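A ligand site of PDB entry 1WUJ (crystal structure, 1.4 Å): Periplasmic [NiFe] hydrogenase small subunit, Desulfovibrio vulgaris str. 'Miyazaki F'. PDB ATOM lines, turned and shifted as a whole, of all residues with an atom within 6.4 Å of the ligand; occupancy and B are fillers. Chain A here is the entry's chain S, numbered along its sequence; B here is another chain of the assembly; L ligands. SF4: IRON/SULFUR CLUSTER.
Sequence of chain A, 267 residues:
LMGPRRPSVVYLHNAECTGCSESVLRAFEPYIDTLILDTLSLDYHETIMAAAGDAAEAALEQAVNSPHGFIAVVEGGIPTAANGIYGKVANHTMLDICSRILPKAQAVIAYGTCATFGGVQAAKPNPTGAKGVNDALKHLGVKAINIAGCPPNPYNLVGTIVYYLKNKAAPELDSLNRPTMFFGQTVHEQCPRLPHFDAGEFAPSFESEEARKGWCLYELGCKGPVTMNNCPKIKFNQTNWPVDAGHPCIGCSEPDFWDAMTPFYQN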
ATOM      1  N   ALA A  15     -19.775  21.901 -33.031  1.00  0.00           N
ATOM      2  CA  ALA A  15     -19.041  21.914 -31.799  1.00  0.00           C
ATOM      3  C   ALA A  15     -19.877  21.092 -30.833  1.00  0.00           C
ATOM      4  O   ALA A  15     -20.880  21.550 -30.308  1.00  0.00           O
ATOM      5  CB  ALA A  15     -18.832  23.302 -31.280  1.00  0.00           C
ATOM      6  N   GLU A  16     -19.423  19.843 -30.678  1.00  0.00           N
ATOM      7  CA  GLU A  16     -20.164  18.815 -29.977  1.00  0.00           C
ATOM      8  C   GLU A  16     -19.236  17.780 -29.366  1.00  0.00           C
ATOM      9  O   GLU A  16     -18.054  17.754 -29.656  1.00  0.00           O
ATOM     10  CB  GLU A  16     -21.177  18.135 -30.931  1.00  0.00           C
ATOM     11  CG  GLU A  16     -20.632  17.853 -32.307  1.00  0.00           C
ATOM     12  CD  GLU A  16     -19.823  16.576 -32.425  1.00  0.00           C
ATOM     13  OE1 GLU A  16     -20.202  15.571 -31.781  1.00  0.00           O
ATOM     14  OE2 GLU A  16     -18.820  16.591 -33.164  1.00  0.00           O
ATOM     15  N   CYS A  17     -19.822  16.934 -28.513  1.00  0.00           N
ATOM     16  CA  CYS A  17     -19.090  15.894 -27.812  1.00  0.00           C
ATOM     17  C   CYS A  17     -19.455  14.497 -28.284  1.00  0.00           C
ATOM     18  O   CYS A  17     -18.899  13.530 -27.745  1.00  0.00           O
ATOM     19  CB  CYS A  17     -19.341  15.977 -26.317  1.00  0.00           C
ATOM     20  SG  CYS A  17     -20.912  15.249 -25.725  1.00  0.00           S
ATOM     21  N   THR A  18     -20.361  14.408 -29.249  1.00  0.00           N
ATOM     22  CA  THR A  18     -20.853  13.158 -29.850  1.00  0.00           C
ATOM     23  C   THR A  18     -21.797  12.410 -28.897  1.00  0.00           C
ATOM     24  O   THR A  18     -22.277  11.331 -29.250  1.00  0.00           O
ATOM     25  CB  THR A  18     -19.692  12.336 -30.424  1.00  0.00           C
ATOM     26  OG1 THR A  18     -18.879  13.212 -31.259  1.00  0.00           O
ATOM     27  CG2 THR A  18     -20.161  11.201 -31.327  1.00  0.00           C
ATOM     28  N   GLY A  19     -22.081  13.000 -27.721  1.00  0.00           N
ATOM     29  CA  GLY A  19     -23.039  12.395 -26.822  1.00  0.00           C
ATOM     30  C   GLY A  19     -24.432  12.352 -27.388  1.00  0.00           C
ATOM     31  O   GLY A  19     -25.242  11.482 -27.088  1.00  0.00           O
ATOM     32  N   CYS A  20     -24.751  13.327 -28.232  1.00  0.00           N
ATOM     33  CA  CYS A  20     -26.079  13.346 -28.864  1.00  0.00           C
ATOM     34  C   CYS A  20     -26.153  12.219 -29.895  1.00  0.00           C
ATOM     35  O   CYS A  20     -27.124  11.449 -29.965  1.00  0.00           O
ATOM     36  CB  CYS A  20     -26.481  14.686 -29.483  1.00  0.00           C
ATOM     37  SG  CYS A  20     -26.870  15.935 -28.202  1.00  0.00           S
ATOM     38  N   SER A  21     -25.092  12.024 -30.705  1.00  0.00           N
ATOM     39  CA  SER A  21     -25.067  10.865 -31.617  1.00  0.00           C
ATOM     40  C   SER A  21     -25.196   9.546 -30.847  1.00  0.00           C
ATOM     41  O   SER A  21     -25.927   8.630 -31.247  1.00  0.00           O
ATOM     42  CB  SER A  21     -23.748  10.828 -32.394  1.00  0.00           C
ATOM     43  OG  SER A  21     -23.743  11.769 -33.463  1.00  0.00           O
ATOM     44  N   GLU A  75     -26.112  18.285 -34.692  1.00  0.00           N
ATOM     45  CA  GLU A  75     -25.549  18.159 -33.361  1.00  0.00           C
ATOM     46  C   GLU A  75     -24.438  19.194 -33.163  1.00  0.00           C
ATOM     47  O   GLU A  75     -23.576  19.287 -34.052  1.00  0.00           O
ATOM     48  CB  GLU A  75     -24.982  16.744 -33.165  1.00  0.00           C
ATOM     49  CG  GLU A  75     -24.306  16.412 -31.856  1.00  0.00           C
ATOM     50  CD  GLU A  75     -23.966  14.906 -31.731  1.00  0.00           C
ATOM     51  OE1 GLU A  75     -23.471  14.515 -30.657  1.00  0.00           O
ATOM     52  OE2 GLU A  75     -24.235  14.208 -32.734  1.00  0.00           O
ATOM     53  N   GLY A  76     -24.426  19.926 -32.045  1.00  0.00           N
ATOM     54  CA  GLY A  76     -23.398  20.853 -31.707  1.00  0.00           C
ATOM     55  C   GLY A  76     -23.731  22.296 -32.062  1.00  0.00           C
ATOM     56  O   GLY A  76     -24.491  22.632 -32.959  1.00  0.00           O
ATOM     57  N   GLY A  77     -23.132  23.191 -31.300  1.00  0.00           N
ATOM     58  CA  GLY A  77     -23.206  24.631 -31.492  1.00  0.00           C
ATOM     59  C   GLY A  77     -22.314  25.061 -32.647  1.00  0.00           C
ATOM     60  O   GLY A  77     -21.393  24.313 -33.015  1.00  0.00           O
ATOM     61  N   TYR A 111     -30.561  18.983 -32.606  1.00  0.00           N
ATOM     62  CA  TYR A 111     -30.640  17.901 -31.636  1.00  0.00           C
ATOM     63  C   TYR A 111     -29.580  18.091 -30.562  1.00  0.00           C
ATOM     64  O   TYR A 111     -28.391  18.044 -30.896  1.00  0.00           O
ATOM     65  CB  TYR A 111     -30.537  16.561 -32.345  1.00  0.00           C
ATOM     66  CG  TYR A 111     -30.724  15.371 -31.413  1.00  0.00           C
ATOM     67  CD1 TYR A 111     -31.942  15.203 -30.748  1.00  0.00           C
ATOM     68  CD2 TYR A 111     -29.712  14.453 -31.200  1.00  0.00           C
ATOM     69  CE1 TYR A 111     -32.162  14.148 -29.897  1.00  0.00           C
ATOM     70  CE2 TYR A 111     -29.947  13.400 -30.325  1.00  0.00           C
ATOM     71  CZ  TYR A 111     -31.148  13.229 -29.675  1.00  0.00           C
ATOM     72  OH  TYR A 111     -31.411  12.200 -28.803  1.00  0.00           O
ATOM     73  N   GLY A 112     -30.028  18.360 -29.333  1.00  0.00           N
ATOM     74  CA  GLY A 112     -29.239  18.606 -28.171  1.00  0.00           C
ATOM     75  C   GLY A 112     -29.091  20.082 -27.861  1.00  0.00           C
ATOM     76  O   GLY A 112     -29.102  20.904 -28.764  1.00  0.00           O
ATOM     77  N   THR A 113     -28.926  20.331 -26.576  1.00  0.00           N
ATOM     78  CA  THR A 113     -28.813  21.701 -26.105  1.00  0.00           C
ATOM     79  C   THR A 113     -27.729  22.492 -26.804  1.00  0.00           C
ATOM     80  O   THR A 113     -27.899  23.703 -26.968  1.00  0.00           O
ATOM     81  CB  THR A 113     -28.620  21.655 -24.588  1.00  0.00           C
ATOM     82  OG1 THR A 113     -29.864  21.135 -24.091  1.00  0.00           O
ATOM     83  CG2 THR A 113     -28.386  23.040 -23.972  1.00  0.00           C
ATOM     84  N   CYS A 114     -26.636  21.882 -27.221  1.00  0.00           N
ATOM     85  CA  CYS A 114     -25.628  22.642 -27.963  1.00  0.00           C
ATOM     86  C   CYS A 114     -26.186  23.161 -29.276  1.00  0.00           C
ATOM     87  O   CYS A 114     -26.056  24.352 -29.555  1.00  0.00           O
ATOM     88  CB  CYS A 114     -24.404  21.784 -28.265  1.00  0.00           C
ATOM     89  SG  CYS A 114     -23.438  21.354 -26.782  1.00  0.00           S
ATOM     90  N   ALA A 115     -26.785  22.286 -30.089  1.00  0.00           N
ATOM     91  CA  ALA A 115     -27.379  22.780 -31.321  1.00  0.00           C
ATOM     92  C   ALA A 115     -28.585  23.676 -31.095  1.00  0.00           C
ATOM     93  O   ALA A 115     -28.852  24.603 -31.912  1.00  0.00           O
ATOM     94  CB  ALA A 115     -27.783  21.577 -32.180  1.00  0.00           C
ATOM     95  N   GLY A 119     -25.109  25.613 -25.831  1.00  0.00           N
ATOM     96  CA  GLY A 119     -24.577  24.581 -24.978  1.00  0.00           C
ATOM     97  C   GLY A 119     -23.262  24.836 -24.295  1.00  0.00           C
ATOM     98  O   GLY A 119     -22.933  25.985 -24.006  1.00  0.00           O
ATOM     99  N   VAL A 120     -22.485  23.788 -23.997  1.00  0.00           N
ATOM    100  CA  VAL A 120     -21.417  23.846 -23.032  1.00  0.00           C
ATOM    101  C   VAL A 120     -20.337  24.810 -23.508  1.00  0.00           C
ATOM    102  O   VAL A 120     -19.809  25.593 -22.721  1.00  0.00           O
ATOM    103  CB  VAL A 120     -20.846  22.432 -22.693  1.00  0.00           C
ATOM    104  CG1 VAL A 120     -20.121  21.824 -23.885  1.00  0.00           C
ATOM    105  CG2 VAL A 120     -19.967  22.486 -21.444  1.00  0.00           C
ATOM    106  N   GLN A 121     -19.986  24.827 -24.778  1.00  0.00           N
ATOM    107  CA  GLN A 121     -18.923  25.713 -25.284  1.00  0.00           C
ATOM    108  C   GLN A 121     -19.440  27.162 -25.336  1.00  0.00           C
ATOM    109  O   GLN A 121     -18.634  28.064 -25.459  1.00  0.00           O
ATOM    110  CB  GLN A 121     -18.360  25.287 -26.637  1.00  0.00           C
ATOM    111  CG  GLN A 121     -19.398  25.124 -27.757  1.00  0.00           C
ATOM    112  CD  GLN A 121     -20.050  23.757 -27.725  1.00  0.00           C
ATOM    113  OE1 GLN A 121     -19.383  22.722 -27.627  1.00  0.00           O
ATOM    114  NE2 GLN A 121     -21.386  23.690 -27.801  1.00  0.00           N
ATOM    115  N   GLY A 149     -31.712  19.026 -24.424  1.00  0.00           N
ATOM    116  CA  GLY A 149     -31.191  18.106 -23.463  1.00  0.00           C
ATOM    117  C   GLY A 149     -29.711  17.799 -23.782  1.00  0.00           C
ATOM    118  O   GLY A 149     -29.286  18.018 -24.910  1.00  0.00           O
ATOM    119  N   CYS A 150     -29.028  17.272 -22.758  1.00  0.00           N
ATOM    120  CA  CYS A 150     -27.588  17.133 -22.867  1.00  0.00           C
ATOM    121  C   CYS A 150     -27.109  15.742 -22.412  1.00  0.00           C
ATOM    122  O   CYS A 150     -26.433  15.569 -21.398  1.00  0.00           O
ATOM    123  CB  CYS A 150     -26.914  18.260 -22.055  1.00  0.00           C
ATOM    124  SG  CYS A 150     -25.169  18.523 -22.404  1.00  0.00           S
ATOM    125  N   PRO A 151     -27.382  14.723 -23.216  1.00  0.00           N
ATOM    126  CA  PRO A 151     -28.162  14.767 -24.455  1.00  0.00           C
ATOM    127  C   PRO A 151     -29.661  14.572 -24.237  1.00  0.00           C
ATOM    128  O   PRO A 151     -30.097  14.183 -23.152  1.00  0.00           O
ATOM    129  CB  PRO A 151     -27.607  13.570 -25.220  1.00  0.00           C
ATOM    130  CG  PRO A 151     -27.346  12.584 -24.145  1.00  0.00           C
ATOM    131  CD  PRO A 151     -26.854  13.365 -22.958  1.00  0.00           C
ATOM    132  N   PRO A 152     -30.441  14.859 -25.275  1.00  0.00           N
ATOM    133  CA  PRO A 152     -31.882  14.656 -25.195  1.00  0.00           C
ATOM    134  C   PRO A 152     -32.188  13.164 -25.045  1.00  0.00           C
ATOM    135  O   PRO A 152     -31.363  12.308 -25.279  1.00  0.00           O
ATOM    136  CB  PRO A 152     -32.412  15.130 -26.577  1.00  0.00           C
ATOM    137  CG  PRO A 152     -31.305  16.020 -27.073  1.00  0.00           C
ATOM    138  CD  PRO A 152     -30.046  15.334 -26.616  1.00  0.00           C
ATOM    139  N   TRP A 258     -25.802  26.166 -18.335  1.00  0.00           N
ATOM    140  CA  TRP A 258     -24.488  26.109 -17.700  1.00  0.00           C
ATOM    141  C   TRP A 258     -24.227  27.321 -16.796  1.00  0.00           C
ATOM    142  O   TRP A 258     -23.505  27.243 -15.811  1.00  0.00           O
ATOM    143  CB  TRP A 258     -23.396  26.029 -18.783  1.00  0.00           C
ATOM    144  CG  TRP A 258     -23.565  24.775 -19.588  1.00  0.00           C
ATOM    145  CD1 TRP A 258     -24.086  24.614 -20.844  1.00  0.00           C
ATOM    146  CD2 TRP A 258     -23.194  23.459 -19.146  1.00  0.00           C
ATOM    147  NE1 TRP A 258     -24.066  23.267 -21.213  1.00  0.00           N
ATOM    148  CE2 TRP A 258     -23.520  22.567 -20.191  1.00  0.00           C
ATOM    149  CE3 TRP A 258     -22.633  22.939 -17.989  1.00  0.00           C
ATOM    150  CZ2 TRP A 258     -23.303  21.167 -20.115  1.00  0.00           C
ATOM    151  CZ3 TRP A 258     -22.419  21.590 -17.911  1.00  0.00           C
ATOM    152  CH2 TRP A 258     -22.750  20.719 -18.944  1.00  0.00           C
ATOM    153  N   ARG B  41     -13.135  23.925 -28.251  1.00  0.00           N
ATOM    154  CA  ARG B  41     -14.266  24.421 -27.467  1.00  0.00           C
ATOM    155  C   ARG B  41     -13.806  25.256 -26.271  1.00  0.00           C
ATOM    156  O   ARG B  41     -14.483  26.205 -25.906  1.00  0.00           O
ATOM    157  CB  ARG B  41     -15.135  23.258 -26.954  1.00  0.00           C
ATOM    158  CG  ARG B  41     -15.892  22.604 -28.104  1.00  0.00           C
ATOM    159  CD  ARG B  41     -16.706  21.351 -27.782  1.00  0.00           C
ATOM    160  NE  ARG B  41     -15.732  20.338 -27.336  1.00  0.00           N
ATOM    161  CZ  ARG B  41     -16.013  19.342 -26.511  1.00  0.00           C
ATOM    162  NH1 ARG B  41     -17.229  19.141 -26.032  1.00  0.00           N
ATOM    163  NH2 ARG B  41     -15.027  18.509 -26.155  1.00  0.00           N
ATOM    164  N   ARG B  61     -18.972  16.643 -20.458  1.00  0.00           N
ATOM    165  CA  ARG B  61     -19.315  17.012 -21.827  1.00  0.00           C
ATOM    166  C   ARG B  61     -18.081  17.217 -22.701  1.00  0.00           C
ATOM    167  O   ARG B  61     -18.204  17.629 -23.876  1.00  0.00           O
ATOM    168  CB  ARG B  61     -20.207  18.268 -21.824  1.00  0.00           C
ATOM    169  CG  ARG B  61     -21.654  17.986 -21.559  1.00  0.00           C
ATOM    170  CD  ARG B  61     -21.894  17.421 -20.176  1.00  0.00           C
ATOM    171  NE  ARG B  61     -23.327  17.147 -20.027  1.00  0.00           N
ATOM    172  CZ  ARG B  61     -23.886  16.682 -18.934  1.00  0.00           C
ATOM    173  NH1 ARG B  61     -23.172  16.475 -17.827  1.00  0.00           N
ATOM    174  NH2 ARG B  61     -25.181  16.419 -18.943  1.00  0.00           N
ATOM    175  N   THR B  62     -16.901  16.924 -22.184  1.00  0.00           N
ATOM    176  CA  THR B  62     -15.743  16.777 -23.048  1.00  0.00           C
ATOM    177  C   THR B  62     -16.045  15.750 -24.134  1.00  0.00           C
ATOM    178  O   THR B  62     -15.627  15.940 -25.271  1.00  0.00           O
ATOM    179  CB  THR B  62     -14.499  16.326 -22.273  1.00  0.00           C
ATOM    180  OG1 THR B  62     -14.121  17.362 -21.350  1.00  0.00           O
ATOM    181  CG2 THR B  62     -13.355  16.069 -23.219  1.00  0.00           C
ATOM    182  N   CYS B  63     -16.736  14.674 -23.704  1.00  0.00           N
ATOM    183  CA  CYS B  63     -16.971  13.599 -24.662  1.00  0.00           C
ATOM    184  C   CYS B  63     -18.125  12.684 -24.259  1.00  0.00           C
ATOM    185  O   CYS B  63     -18.200  12.298 -23.097  1.00  0.00           O
ATOM    186  CB  CYS B  63     -15.680  12.794 -24.762  1.00  0.00           C
ATOM    187  SG  CYS B  63     -15.805  11.541 -26.103  1.00  0.00           S
ATOM    188  N   GLY B  64     -18.944  12.382 -25.261  1.00  0.00           N
ATOM    189  CA  GLY B  64     -20.106  11.547 -25.059  1.00  0.00           C
ATOM    190  C   GLY B  64     -19.890  10.124 -25.520  1.00  0.00           C
ATOM    191  O   GLY B  64     -20.734   9.258 -25.273  1.00  0.00           O
ATOM    192  N   PRO B 216     -26.263   8.407 -22.653  1.00  0.00           N
ATOM    193  CA  PRO B 216     -25.025   9.054 -22.240  1.00  0.00           C
ATOM    194  C   PRO B 216     -25.283  10.064 -21.141  1.00  0.00           C
ATOM    195  O   PRO B 216     -26.308  10.614 -20.835  1.00  0.00           O
ATOM    196  CB  PRO B 216     -24.539   9.779 -23.514  1.00  0.00           C
ATOM    197  CG  PRO B 216     -25.261   9.110 -24.642  1.00  0.00           C
ATOM    198  CD  PRO B 216     -26.618   8.798 -24.040  1.00  0.00           C
ATOM    199  N   HIS B 217     -24.278  10.310 -20.362  1.00  0.00           N
ATOM    200  CA  HIS B 217     -23.812  11.344 -19.460  1.00  0.00           C
ATOM    201  C   HIS B 217     -24.444  10.982 -18.131  1.00  0.00           C
ATOM    202  O   HIS B 217     -25.534  11.429 -17.780  1.00  0.00           O
ATOM    203  CB  HIS B 217     -24.104  12.761 -19.970  1.00  0.00           C
ATOM    204  CG  HIS B 217     -23.125  13.241 -21.012  1.00  0.00           C
ATOM    205  ND1 HIS B 217     -23.236  14.248 -21.916  1.00  0.00           N
ATOM    206  CD2 HIS B 217     -21.876  12.682 -21.249  1.00  0.00           C
ATOM    207  CE1 HIS B 217     -22.130  14.330 -22.649  1.00  0.00           C
ATOM    208  NE2 HIS B 217     -21.308  13.387 -22.266  1.00  0.00           N
HETATM  209 FE1  SF4 L   1     -22.641  16.756 -26.004  1.00  0.00          FE
HETATM  210 FE2  SF4 L   1     -23.796  19.082 -26.629  1.00  0.00          FE
HETATM  211 FE3  SF4 L   1     -24.601  17.799 -24.498  1.00  0.00          FE
HETATM  212 FE4  SF4 L   1     -25.166  16.758 -26.971  1.00  0.00          FE
HETATM  213  S1  SF4 L   1     -26.008  18.700 -26.087  1.00  0.00           S
HETATM  214  S2  SF4 L   1     -24.458  15.608 -25.094  1.00  0.00           S
HETATM  215  S3  SF4 L   1     -23.288  17.432 -28.135  1.00  0.00           S
HETATM  216  S4  SF4 L   1     -22.438  18.663 -24.830  1.00  0.00           S
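N of Cys 17 lies close to S3 of the ligand, 3.5 Å away. A sulfur (S1) of the ligand sits close to the backbone NH of Cys 114, at 3.4 Å. An iron atom (FE3) of the ligand is bound by the side-chain sulfur of Cys 150 (2.3 Å). The side-chain sulfur (SG) of Cys 114 is bound to an iron atom (FE2) of the ligand (2.3 Å). SG of Cys 20 is bound to FE4 of the ligand (2.3 Å). ND1 of His 217 of chain B sits close to S2 of the ligand (3.7 Å). A sulfur (S1) of the ligand sits close to the backbone NH (N) of Thr 113 (3.4 Å). An iron atom (FE1) of the ligand is bound by the side-chain sulfur of Cys 17 (2.3 Å).
O of Tyr 111 sits close to SG of Cys 20 (3.7 Å). O of Cys 150 lies within hydrogen-bond range of ND1 of His 217 of chain B, at 3.5 Å. O of Cys 150 is in hydrogen-bond range of NH2 of Arg 61 of chain B (2.9 Å). N of Gly 64 of chain B is in hydrogen-bond range of O of Cys 17 (2.7 Å). The backbone NH of Gly 149 lies within hydrogen-bond range of the side-chain hydroxyl of Thr 113. The backbone NH of Cys 20 is in hydrogen-bond range of the side-chain carboxylate of Glu 75, 3.0 Å away. The side-chain sulfur (SG) of Cys 114 sits close to the side-chain amide nitrogen (NE2) of Gln 121, at 3.3 Å. O of Cys 63 of chain B is in hydrogen-bond range of NE2 of His 217 of chain B.
A sulfur (S1) of the ligand sits close to the backbone carbonyl oxygen (O) of Gly 149, at 3.5 Å. N of Pro 151 lies close to S2 of the ligand, 3.6 Å away. Residues that only touch the ligand: Arg 61 of chain B (3.4 Å), Glu 16 (3.6 Å), Gly 112 (3.8 Å), Glu 75 (3.9 Å) and Gly 19 (3.9 Å). Hydrophobic or aromatic side chains within 4 Å of the ligand: Pro 151 and His 217 of chain B. Of the 30 residues printed, 13 come within 4 Å of the ligand.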
